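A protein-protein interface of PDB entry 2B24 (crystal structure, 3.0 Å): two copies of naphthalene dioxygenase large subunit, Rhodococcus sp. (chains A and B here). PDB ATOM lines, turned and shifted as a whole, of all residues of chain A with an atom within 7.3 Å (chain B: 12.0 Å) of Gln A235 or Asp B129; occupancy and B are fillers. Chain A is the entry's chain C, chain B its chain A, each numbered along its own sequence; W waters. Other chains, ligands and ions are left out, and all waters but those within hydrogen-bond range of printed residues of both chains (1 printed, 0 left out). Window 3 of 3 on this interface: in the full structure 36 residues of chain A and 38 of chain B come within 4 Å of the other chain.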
ATOM      1  N   MET A 218     -23.158 -31.661  -3.628  1.00  0.00           N
ATOM      2  CA  MET A 218     -24.617 -31.678  -3.463  1.00  0.00           C
ATOM      3  C   MET A 218     -25.216 -33.002  -3.016  1.00  0.00           C
ATOM      4  O   MET A 218     -26.188 -33.005  -2.273  1.00  0.00           O
ATOM      5  CB  MET A 218     -25.354 -31.156  -4.701  1.00  0.00           C
ATOM      6  CG  MET A 218     -24.655 -31.391  -6.011  1.00  0.00           C
ATOM      7  SD  MET A 218     -24.981 -30.076  -7.195  1.00  0.00           S
ATOM      8  CE  MET A 218     -26.732 -30.118  -7.227  1.00  0.00           C
ATOM      9  N   PRO A 231     -23.535 -24.502   0.159  1.00  0.00           N
ATOM     10  CA  PRO A 231     -24.362 -23.758  -0.802  1.00  0.00           C
ATOM     11  C   PRO A 231     -25.634 -24.520  -1.223  1.00  0.00           C
ATOM     12  O   PRO A 231     -25.524 -25.637  -1.752  1.00  0.00           O
ATOM     13  CB  PRO A 231     -23.423 -23.586  -1.999  1.00  0.00           C
ATOM     14  CG  PRO A 231     -22.055 -23.608  -1.411  1.00  0.00           C
ATOM     15  CD  PRO A 231     -22.124 -24.576  -0.268  1.00  0.00           C
ATOM     16  N   PRO A 232     -26.810 -23.925  -0.986  1.00  0.00           N
ATOM     17  CA  PRO A 232     -28.108 -24.555  -1.300  1.00  0.00           C
ATOM     18  C   PRO A 232     -28.484 -24.558  -2.789  1.00  0.00           C
ATOM     19  O   PRO A 232     -29.364 -25.325  -3.184  1.00  0.00           O
ATOM     20  CB  PRO A 232     -29.117 -23.694  -0.524  1.00  0.00           C
ATOM     21  CG  PRO A 232     -28.289 -22.792   0.334  1.00  0.00           C
ATOM     22  CD  PRO A 232     -26.989 -22.593  -0.386  1.00  0.00           C
ATOM     23  N   ASP A 233     -27.838 -23.706  -3.582  1.00  0.00           N
ATOM     24  CA  ASP A 233     -28.177 -23.563  -4.993  1.00  0.00           C
ATOM     25  C   ASP A 233     -27.487 -24.646  -5.825  1.00  0.00           C
ATOM     26  O   ASP A 233     -26.255 -24.690  -5.889  1.00  0.00           O
ATOM     27  CB  ASP A 233     -27.800 -22.153  -5.489  1.00  0.00           C
ATOM     28  CG  ASP A 233     -28.029 -21.965  -6.990  1.00  0.00           C
ATOM     29  OD1 ASP A 233     -29.033 -22.482  -7.533  1.00  0.00           O
ATOM     30  OD2 ASP A 233     -27.251 -21.304  -7.708  1.00  0.00           O
ATOM     31  N   PRO A 234     -28.275 -25.509  -6.469  1.00  0.00           N
ATOM     32  CA  PRO A 234     -27.738 -26.650  -7.229  1.00  0.00           C
ATOM     33  C   PRO A 234     -26.772 -26.282  -8.347  1.00  0.00           C
ATOM     34  O   PRO A 234     -26.165 -27.178  -8.941  1.00  0.00           O
ATOM     35  CB  PRO A 234     -28.994 -27.288  -7.824  1.00  0.00           C
ATOM     36  CG  PRO A 234     -30.070 -26.886  -6.906  1.00  0.00           C
ATOM     37  CD  PRO A 234     -29.746 -25.481  -6.495  1.00  0.00           C
ATOM     38  N   GLN A 235     -26.640 -24.989  -8.637  1.00  0.00           N
ATOM     39  CA  GLN A 235     -25.738 -24.525  -9.690  1.00  0.00           C
ATOM     40  C   GLN A 235     -24.752 -23.509  -9.114  1.00  0.00           C
ATOM     41  O   GLN A 235     -24.354 -22.548  -9.794  1.00  0.00           O
ATOM     42  CB  GLN A 235     -26.518 -23.957 -10.895  1.00  0.00           C
ATOM     43  CG  GLN A 235     -27.918 -23.407 -10.573  1.00  0.00           C
ATOM     44  CD  GLN A 235     -28.537 -22.623 -11.735  1.00  0.00           C
ATOM     45  OE1 GLN A 235     -28.875 -21.435 -11.587  1.00  0.00           O
ATOM     46  NE2 GLN A 235     -28.694 -23.286 -12.884  1.00  0.00           N
ATOM     47  N   PHE A 236     -24.354 -23.739  -7.860  1.00  0.00           N
ATOM     48  CA  PHE A 236     -23.416 -22.852  -7.171  1.00  0.00           C
ATOM     49  C   PHE A 236     -21.990 -22.889  -7.744  1.00  0.00           C
ATOM     50  O   PHE A 236     -21.251 -21.910  -7.635  1.00  0.00           O
ATOM     51  CB  PHE A 236     -23.419 -23.129  -5.663  1.00  0.00           C
ATOM     52  CG  PHE A 236     -22.453 -24.215  -5.226  1.00  0.00           C
ATOM     53  CD1 PHE A 236     -21.170 -23.889  -4.770  1.00  0.00           C
ATOM     54  CD2 PHE A 236     -22.832 -25.550  -5.250  1.00  0.00           C
ATOM     55  CE1 PHE A 236     -20.280 -24.877  -4.363  1.00  0.00           C
ATOM     56  CE2 PHE A 236     -21.951 -26.542  -4.847  1.00  0.00           C
ATOM     57  CZ  PHE A 236     -20.670 -26.205  -4.403  1.00  0.00           C
ATOM     58  N   ALA A 237     -21.618 -24.014  -8.349  1.00  0.00           N
ATOM     59  CA  ALA A 237     -20.292 -24.176  -8.933  1.00  0.00           C
ATOM     60  C   ALA A 237     -20.173 -23.481 -10.273  1.00  0.00           C
ATOM     61  O   ALA A 237     -19.064 -23.149 -10.700  1.00  0.00           O
ATOM     62  CB  ALA A 237     -19.964 -25.628  -9.088  1.00  0.00           C
ATOM     63  N   LEU A 238     -21.317 -23.275 -10.929  1.00  0.00           N
ATOM     64  CA  LEU A 238     -21.390 -22.599 -12.223  1.00  0.00           C
ATOM     65  C   LEU A 238     -20.775 -21.199 -12.168  1.00  0.00           C
ATOM     66  O   LEU A 238     -20.196 -20.729 -13.155  1.00  0.00           O
ATOM     67  CB  LEU A 238     -22.844 -22.531 -12.678  1.00  0.00           C
ATOM     68  CG  LEU A 238     -23.230 -23.304 -13.940  1.00  0.00           C
ATOM     69  CD1 LEU A 238     -22.799 -24.770 -13.908  1.00  0.00           C
ATOM     70  CD2 LEU A 238     -24.734 -23.194 -14.149  1.00  0.00           C
ATOM     71  N   TYR A 239     -20.908 -20.546 -11.012  1.00  0.00           N
ATOM     72  CA  TYR A 239     -20.160 -19.331 -10.718  1.00  0.00           C
ATOM     73  C   TYR A 239     -18.793 -19.731 -10.172  1.00  0.00           C
ATOM     74  O   TYR A 239     -18.529 -19.631  -8.970  1.00  0.00           O
ATOM     75  CB  TYR A 239     -20.910 -18.457  -9.711  1.00  0.00           C
ATOM     76  CG  TYR A 239     -22.403 -18.413  -9.934  1.00  0.00           C
ATOM     77  CD1 TYR A 239     -23.251 -19.300  -9.259  1.00  0.00           C
ATOM     78  CD2 TYR A 239     -22.973 -17.491 -10.819  1.00  0.00           C
ATOM     79  CE1 TYR A 239     -24.630 -19.269  -9.452  1.00  0.00           C
ATOM     80  CE2 TYR A 239     -24.352 -17.453 -11.029  1.00  0.00           C
ATOM     81  CZ  TYR A 239     -25.174 -18.344 -10.336  1.00  0.00           C
ATOM     82  OH  TYR A 239     -26.535 -18.328 -10.524  1.00  0.00           O
ATOM     83  N   GLY A 240     -17.936 -20.197 -11.076  1.00  0.00           N
ATOM     84  CA  GLY A 240     -16.596 -20.628 -10.735  1.00  0.00           C
ATOM     85  C   GLY A 240     -15.702 -20.736 -11.952  1.00  0.00           C
ATOM     86  O   GLY A 240     -16.065 -20.281 -13.028  1.00  0.00           O
ATOM     87  N   PRO A 257     -23.071 -16.068  -6.197  1.00  0.00           N
ATOM     88  CA  PRO A 257     -23.930 -15.577  -7.286  1.00  0.00           C
ATOM     89  C   PRO A 257     -23.922 -14.045  -7.384  1.00  0.00           C
ATOM     90  O   PRO A 257     -23.639 -13.400  -6.371  1.00  0.00           O
ATOM     91  CB  PRO A 257     -25.322 -16.063  -6.871  1.00  0.00           C
ATOM     92  CG  PRO A 257     -25.075 -17.232  -6.000  1.00  0.00           C
ATOM     93  CD  PRO A 257     -23.843 -16.874  -5.231  1.00  0.00           C
ATOM     94  N   MET A 397     -17.720 -34.939 -18.298  1.00  0.00           N
ATOM     95  CA  MET A 397     -18.488 -33.749 -17.972  1.00  0.00           C
ATOM     96  C   MET A 397     -18.034 -32.579 -18.821  1.00  0.00           C
ATOM     97  O   MET A 397     -16.908 -32.103 -18.694  1.00  0.00           O
ATOM     98  CB  MET A 397     -18.360 -33.411 -16.494  1.00  0.00           C
ATOM     99  CG  MET A 397     -19.425 -32.501 -15.989  1.00  0.00           C
ATOM    100  SD  MET A 397     -18.990 -31.919 -14.345  1.00  0.00           S
ATOM    101  CE  MET A 397     -19.672 -33.299 -13.379  1.00  0.00           C
ATOM    102  N   VAL A 401     -18.756 -28.962 -24.968  1.00  0.00           N
ATOM    103  CA  VAL A 401     -19.247 -27.710 -24.378  1.00  0.00           C
ATOM    104  C   VAL A 401     -18.095 -26.906 -23.751  1.00  0.00           C
ATOM    105  O   VAL A 401     -18.186 -25.680 -23.599  1.00  0.00           O
ATOM    106  CB  VAL A 401     -20.391 -27.944 -23.325  1.00  0.00           C
ATOM    107  CG1 VAL A 401     -20.414 -26.848 -22.231  1.00  0.00           C
ATOM    108  CG2 VAL A 401     -21.754 -28.026 -24.005  1.00  0.00           C
ATOM    109  N   LEU A 417     -16.616 -22.104 -15.607  1.00  0.00           N
ATOM    110  CA  LEU A 417     -17.565 -22.696 -14.649  1.00  0.00           C
ATOM    111  C   LEU A 417     -16.758 -23.668 -13.783  1.00  0.00           C
ATOM    112  O   LEU A 417     -15.584 -23.901 -14.085  1.00  0.00           O
ATOM    113  CB  LEU A 417     -18.719 -23.399 -15.386  1.00  0.00           C
ATOM    114  CG  LEU A 417     -18.615 -24.833 -15.926  1.00  0.00           C
ATOM    115  CD1 LEU A 417     -19.941 -25.257 -16.560  1.00  0.00           C
ATOM    116  CD2 LEU A 417     -17.464 -25.011 -16.915  1.00  0.00           C
ATOM    117  N   TYR A 419     -18.298 -26.855 -12.818  1.00  0.00           N
ATOM    118  CA  TYR A 419     -18.803 -28.190 -13.127  1.00  0.00           C
ATOM    119  C   TYR A 419     -18.076 -28.734 -14.344  1.00  0.00           C
ATOM    120  O   TYR A 419     -18.605 -28.709 -15.456  1.00  0.00           O
ATOM    121  CB  TYR A 419     -20.310 -28.176 -13.379  1.00  0.00           C
ATOM    122  CG  TYR A 419     -21.159 -28.053 -12.142  1.00  0.00           C
ATOM    123  CD1 TYR A 419     -22.424 -27.498 -12.217  1.00  0.00           C
ATOM    124  CD2 TYR A 419     -20.713 -28.509 -10.908  1.00  0.00           C
ATOM    125  CE1 TYR A 419     -23.230 -27.385 -11.088  1.00  0.00           C
ATOM    126  CE2 TYR A 419     -21.511 -28.406  -9.773  1.00  0.00           C
ATOM    127  CZ  TYR A 419     -22.764 -27.838  -9.870  1.00  0.00           C
ATOM    128  OH  TYR A 419     -23.550 -27.719  -8.752  1.00  0.00           O
ATOM    129  N   HIS B 111     -21.851 -38.582  -6.255  1.00  0.00           N
ATOM    130  CA  HIS B 111     -22.339 -37.431  -7.030  1.00  0.00           C
ATOM    131  C   HIS B 111     -23.870 -37.345  -7.172  1.00  0.00           C
ATOM    132  O   HIS B 111     -24.428 -36.250  -7.330  1.00  0.00           O
ATOM    133  CB  HIS B 111     -21.644 -37.355  -8.390  1.00  0.00           C
ATOM    134  CG  HIS B 111     -20.156 -37.260  -8.295  1.00  0.00           C
ATOM    135  ND1 HIS B 111     -19.342 -38.366  -8.329  1.00  0.00           N
ATOM    136  CD2 HIS B 111     -19.334 -36.195  -8.145  1.00  0.00           C
ATOM    137  CE1 HIS B 111     -18.081 -37.990  -8.220  1.00  0.00           C
ATOM    138  NE2 HIS B 111     -18.048 -36.675  -8.108  1.00  0.00           N
ATOM    139  N   TRP B 113     -25.846 -39.890  -9.070  1.00  0.00           N
ATOM    140  CA  TRP B 113     -26.395 -40.635 -10.199  1.00  0.00           C
ATOM    141  C   TRP B 113     -27.386 -41.680  -9.683  1.00  0.00           C
ATOM    142  O   TRP B 113     -26.985 -42.610  -8.994  1.00  0.00           O
ATOM    143  CB  TRP B 113     -25.283 -41.323 -10.997  1.00  0.00           C
ATOM    144  CG  TRP B 113     -24.443 -40.431 -11.866  1.00  0.00           C
ATOM    145  CD1 TRP B 113     -24.196 -39.106 -11.696  1.00  0.00           C
ATOM    146  CD2 TRP B 113     -23.724 -40.822 -13.032  1.00  0.00           C
ATOM    147  NE1 TRP B 113     -23.368 -38.640 -12.687  1.00  0.00           N
ATOM    148  CE2 TRP B 113     -23.062 -39.679 -13.523  1.00  0.00           C
ATOM    149  CE3 TRP B 113     -23.569 -42.032 -13.723  1.00  0.00           C
ATOM    150  CZ2 TRP B 113     -22.263 -39.707 -14.673  1.00  0.00           C
ATOM    151  CZ3 TRP B 113     -22.768 -42.058 -14.861  1.00  0.00           C
ATOM    152  CH2 TRP B 113     -22.126 -40.902 -15.322  1.00  0.00           C
ATOM    153  N   GLY B 123     -31.378 -40.723 -13.662  1.00  0.00           N
ATOM    154  CA  GLY B 123     -31.191 -39.324 -13.313  1.00  0.00           C
ATOM    155  C   GLY B 123     -29.787 -38.890 -12.944  1.00  0.00           C
ATOM    156  O   GLY B 123     -29.191 -39.414 -11.994  1.00  0.00           O
ATOM    157  N   VAL B 124     -29.274 -37.915 -13.690  1.00  0.00           N
ATOM    158  CA  VAL B 124     -27.978 -37.316 -13.401  1.00  0.00           C
ATOM    159  C   VAL B 124     -28.148 -35.873 -12.927  1.00  0.00           C
ATOM    160  O   VAL B 124     -28.484 -34.983 -13.726  1.00  0.00           O
ATOM    161  CB  VAL B 124     -27.057 -37.329 -14.630  1.00  0.00           C
ATOM    162  CG1 VAL B 124     -25.760 -36.631 -14.325  1.00  0.00           C
ATOM    163  CG2 VAL B 124     -26.797 -38.747 -15.082  1.00  0.00           C
ATOM    164  N   PRO B 125     -27.902 -35.634 -11.639  1.00  0.00           N
ATOM    165  CA  PRO B 125     -27.945 -34.274 -11.085  1.00  0.00           C
ATOM    166  C   PRO B 125     -27.148 -33.289 -11.959  1.00  0.00           C
ATOM    167  O   PRO B 125     -26.066 -33.635 -12.467  1.00  0.00           O
ATOM    168  CB  PRO B 125     -27.281 -34.440  -9.712  1.00  0.00           C
ATOM    169  CG  PRO B 125     -27.565 -35.822  -9.340  1.00  0.00           C
ATOM    170  CD  PRO B 125     -27.553 -36.629 -10.612  1.00  0.00           C
ATOM    171  N   ALA B 126     -27.686 -32.085 -12.138  1.00  0.00           N
ATOM    172  CA  ALA B 126     -27.057 -31.090 -13.006  1.00  0.00           C
ATOM    173  C   ALA B 126     -26.849 -31.627 -14.436  1.00  0.00           C
ATOM    174  O   ALA B 126     -25.730 -31.598 -14.972  1.00  0.00           O
ATOM    175  CB  ALA B 126     -25.722 -30.599 -12.402  1.00  0.00           C
ATOM    176  N   GLY B 127     -27.934 -32.131 -15.030  1.00  0.00           N
ATOM    177  CA  GLY B 127     -27.937 -32.599 -16.404  1.00  0.00           C
ATOM    178  C   GLY B 127     -27.643 -31.453 -17.353  1.00  0.00           C
ATOM    179  O   GLY B 127     -26.743 -31.556 -18.198  1.00  0.00           O
ATOM    180  N   LYS B 128     -28.396 -30.361 -17.211  1.00  0.00           N
ATOM    181  CA  LYS B 128     -28.157 -29.141 -17.995  1.00  0.00           C
ATOM    182  C   LYS B 128     -26.942 -28.370 -17.472  1.00  0.00           C
ATOM    183  O   LYS B 128     -26.080 -27.955 -18.248  1.00  0.00           O
ATOM    184  CB  LYS B 128     -29.392 -28.207 -18.020  1.00  0.00           C
ATOM    185  CG  LYS B 128     -30.519 -28.545 -17.022  1.00  0.00           C
ATOM    186  CD  LYS B 128     -30.163 -28.200 -15.556  1.00  0.00           C
ATOM    187  CE  LYS B 128     -30.120 -29.453 -14.686  1.00  0.00           C
ATOM    188  NZ  LYS B 128     -30.386 -29.114 -13.276  1.00  0.00           N
ATOM    189  N   ASP B 129     -26.883 -28.192 -16.153  1.00  0.00           N
ATOM    190  CA  ASP B 129     -25.862 -27.352 -15.534  1.00  0.00           C
ATOM    191  C   ASP B 129     -24.440 -27.853 -15.789  1.00  0.00           C
ATOM    192  O   ASP B 129     -23.592 -27.086 -16.261  1.00  0.00           O
ATOM    193  CB  ASP B 129     -26.140 -27.166 -14.040  1.00  0.00           C
ATOM    194  CG  ASP B 129     -27.383 -26.308 -13.778  1.00  0.00           C
ATOM    195  OD1 ASP B 129     -28.175 -26.639 -12.865  1.00  0.00           O
ATOM    196  OD2 ASP B 129     -27.652 -25.277 -14.439  1.00  0.00           O
ATOM    197  N   ALA B 130     -24.191 -29.134 -15.518  1.00  0.00           N
ATOM    198  CA  ALA B 130     -22.845 -29.698 -15.656  1.00  0.00           C
ATOM    199  C   ALA B 130     -22.573 -30.223 -17.057  1.00  0.00           C
ATOM    200  O   ALA B 130     -21.636 -29.773 -17.720  1.00  0.00           O
ATOM    201  CB  ALA B 130     -22.613 -30.800 -14.625  1.00  0.00           C
ATOM    202  N   TYR B 131     -23.409 -31.169 -17.495  1.00  0.00           N
ATOM    203  CA  TYR B 131     -23.192 -31.932 -18.727  1.00  0.00           C
ATOM    204  C   TYR B 131     -23.789 -31.280 -19.966  1.00  0.00           C
ATOM    205  O   TYR B 131     -23.450 -31.666 -21.092  1.00  0.00           O
ATOM    206  CB  TYR B 131     -23.781 -33.341 -18.589  1.00  0.00           C
ATOM    207  CG  TYR B 131     -23.081 -34.227 -17.578  1.00  0.00           C
ATOM    208  CD1 TYR B 131     -23.399 -34.150 -16.223  1.00  0.00           C
ATOM    209  CD2 TYR B 131     -22.099 -35.144 -17.976  1.00  0.00           C
ATOM    210  CE1 TYR B 131     -22.762 -34.956 -15.288  1.00  0.00           C
ATOM    211  CE2 TYR B 131     -21.460 -35.960 -17.043  1.00  0.00           C
ATOM    212  CZ  TYR B 131     -21.803 -35.858 -15.701  1.00  0.00           C
ATOM    213  OH  TYR B 131     -21.185 -36.648 -14.762  1.00  0.00           O
ATOM    214  N   GLY B 132     -24.694 -30.323 -19.757  1.00  0.00           N
ATOM    215  CA  GLY B 132     -25.378 -29.633 -20.843  1.00  0.00           C
ATOM    216  C   GLY B 132     -26.186 -30.559 -21.741  1.00  0.00           C
ATOM    217  O   GLY B 132     -26.145 -30.447 -22.975  1.00  0.00           O
ATOM    218  N   ASN B 133     -26.920 -31.478 -21.109  1.00  0.00           N
ATOM    219  CA  ASN B 133     -27.670 -32.547 -21.796  1.00  0.00           C
ATOM    220  C   ASN B 133     -26.871 -33.452 -22.754  1.00  0.00           C
ATOM    221  O   ASN B 133     -27.438 -34.360 -23.369  1.00  0.00           O
ATOM    222  CB  ASN B 133     -28.926 -32.009 -22.498  1.00  0.00           C
ATOM    223  CG  ASN B 133     -29.372 -30.661 -21.960  1.00  0.00           C
ATOM    224  OD1 ASN B 133     -29.297 -29.642 -22.664  1.00  0.00           O
ATOM    225  ND2 ASN B 133     -29.840 -30.644 -20.708  1.00  0.00           N
ATOM    226  N   GLN B 134     -25.563 -33.223 -22.862  1.00  0.00           N
ATOM    227  CA  GLN B 134     -24.724 -33.990 -23.785  1.00  0.00           C
ATOM    228  C   GLN B 134     -24.389 -35.400 -23.280  1.00  0.00           C
ATOM    229  O   GLN B 134     -23.703 -36.171 -23.972  1.00  0.00           O
ATOM    230  CB  GLN B 134     -23.439 -33.217 -24.108  1.00  0.00           C
ATOM    231  CG  GLN B 134     -23.664 -31.782 -24.624  1.00  0.00           C
ATOM    232  CD  GLN B 134     -24.521 -31.735 -25.892  1.00  0.00           C
ATOM    233  OE1 GLN B 134     -24.088 -32.180 -26.964  1.00  0.00           O
ATOM    234  NE2 GLN B 134     -25.741 -31.202 -25.765  1.00  0.00           N
ATOM    235  N   LEU B 135     -24.878 -35.725 -22.077  1.00  0.00           N
ATOM    236  CA  LEU B 135     -24.657 -37.036 -21.468  1.00  0.00           C
ATOM    237  C   LEU B 135     -25.741 -38.014 -21.900  1.00  0.00           C
ATOM    238  O   LEU B 135     -26.921 -37.821 -21.605  1.00  0.00           O
ATOM    239  CB  LEU B 135     -24.587 -36.933 -19.933  1.00  0.00           C
ATOM    240  CG  LEU B 135     -24.611 -38.190 -19.039  1.00  0.00           C
ATOM    241  CD1 LEU B 135     -23.455 -39.151 -19.315  1.00  0.00           C
ATOM    242  CD2 LEU B 135     -24.615 -37.790 -17.572  1.00  0.00           C
ATOM    243  N   LYS B 137     -27.430 -41.308 -21.218  1.00  0.00           N
ATOM    244  CA  LYS B 137     -27.609 -42.169 -20.046  1.00  0.00           C
ATOM    245  C   LYS B 137     -27.526 -43.662 -20.381  1.00  0.00           C
ATOM    246  O   LYS B 137     -26.792 -44.397 -19.723  1.00  0.00           O
ATOM    247  CB  LYS B 137     -28.913 -41.835 -19.311  1.00  0.00           C
ATOM    248  CG  LYS B 137     -28.971 -40.411 -18.761  1.00  0.00           C
ATOM    249  CD  LYS B 137     -30.196 -40.220 -17.873  1.00  0.00           C
ATOM    250  CE  LYS B 137     -30.847 -38.855 -18.073  1.00  0.00           C
ATOM    251  NZ  LYS B 137     -31.274 -38.218 -16.787  1.00  0.00           N
HETATM  252  O   HOH W   1     -27.786 -22.429 -15.791  1.00  0.00           O
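The backbone carbonyl oxygen (O) of Ala B126 sits at hydrogen-bond distance from the backbone NH (N) of Tyr B131, 3.5 Å away.
The side-chain amino group of Lys B128 is in salt-bridge range of the side-chain carboxylate of Asp B129.
The side-chain sulfur (SD) of Met A218 sits at hydrogen-bond distance from the side-chain hydroxyl (OH) of Tyr A419, at 3.2 Å.
The backbone carbonyl oxygen of Pro A234 is in hydrogen-bond range of the side-chain hydroxyl of Tyr A419 (2.7 Å).
The side-chain amide nitrogen (NE2) of Gln A235 lies within hydrogen-bond range of the side-chain carboxylate (OD2) of Asp B129 (2.7 Å).
Gln A235 touches just one residue of chain B: Asp B129 (2.7 Å).
Asp B129 touches just these residues of chain A: Gln A235 and Leu A238.
No residue of chain B comes within 4 Å of Ala A237.
Of chain B, only Asp B129 (3.4 Å) comes within 4 Å of Leu A238.
Tyr A419 touches just one residue of chain B: Ala B130 (3.7 Å).
Of the printed residues of chain A, Ala B130 touches Met A397 and Tyr A419.
Printed residues of chain A within 4 Å of Tyr B131: Met A397.
Pro B125 touches none of the printed residues of chain A.
Val B124 touches none of the printed residues of chain A.
The nearest printed residue of chain A that does not touch Asp B129 is Leu A417 (4.1 Å).
Water W1 lies within hydrogen-bond range of the side-chain carboxylate (OD2) of Asp B129 (3.2 Å) and the side-chain amide nitrogen (NE2) of Gln A235 (3.2 Å).
No position is printed for both chains.
Of the 5 pairs that touch across the chains among the printed residues, none has its exchanged pair printed and touching as well.
Of the 16 printed residues of chain B, 3 touch a printed residue of chain A.
Printed residues of chain B that touch a printed residue of chain A: Asp B129, Ala B130 and Tyr B131.
Hydrophobic or aromatic side chains of chain B within 4 Å of the printed part of chain A: Ala B130 and Tyr B131.
Printed residues of chain A that touch a printed residue of chain B: Gln A235, Leu A238, Met A397 and Tyr A419.
Hydrophobic or aromatic side chains of chain A that line the printed part of chain B: Leu A238, Met A397 and Tyr A419.
Along chain A the printed residues that touch a printed residue of chain B span positions 235 to 419.
Among the printed residues, 5 pairs touch across the chains.
CD1 of Leu A238 touches O of Asp B129 (3.4 Å).
SD of Met A397 touches CB of Ala B130, 3.8 Å away.
Tyr B131 touches Met A397.
Ala B130 touches Tyr A419 (CB to CB, 3.7 Å).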
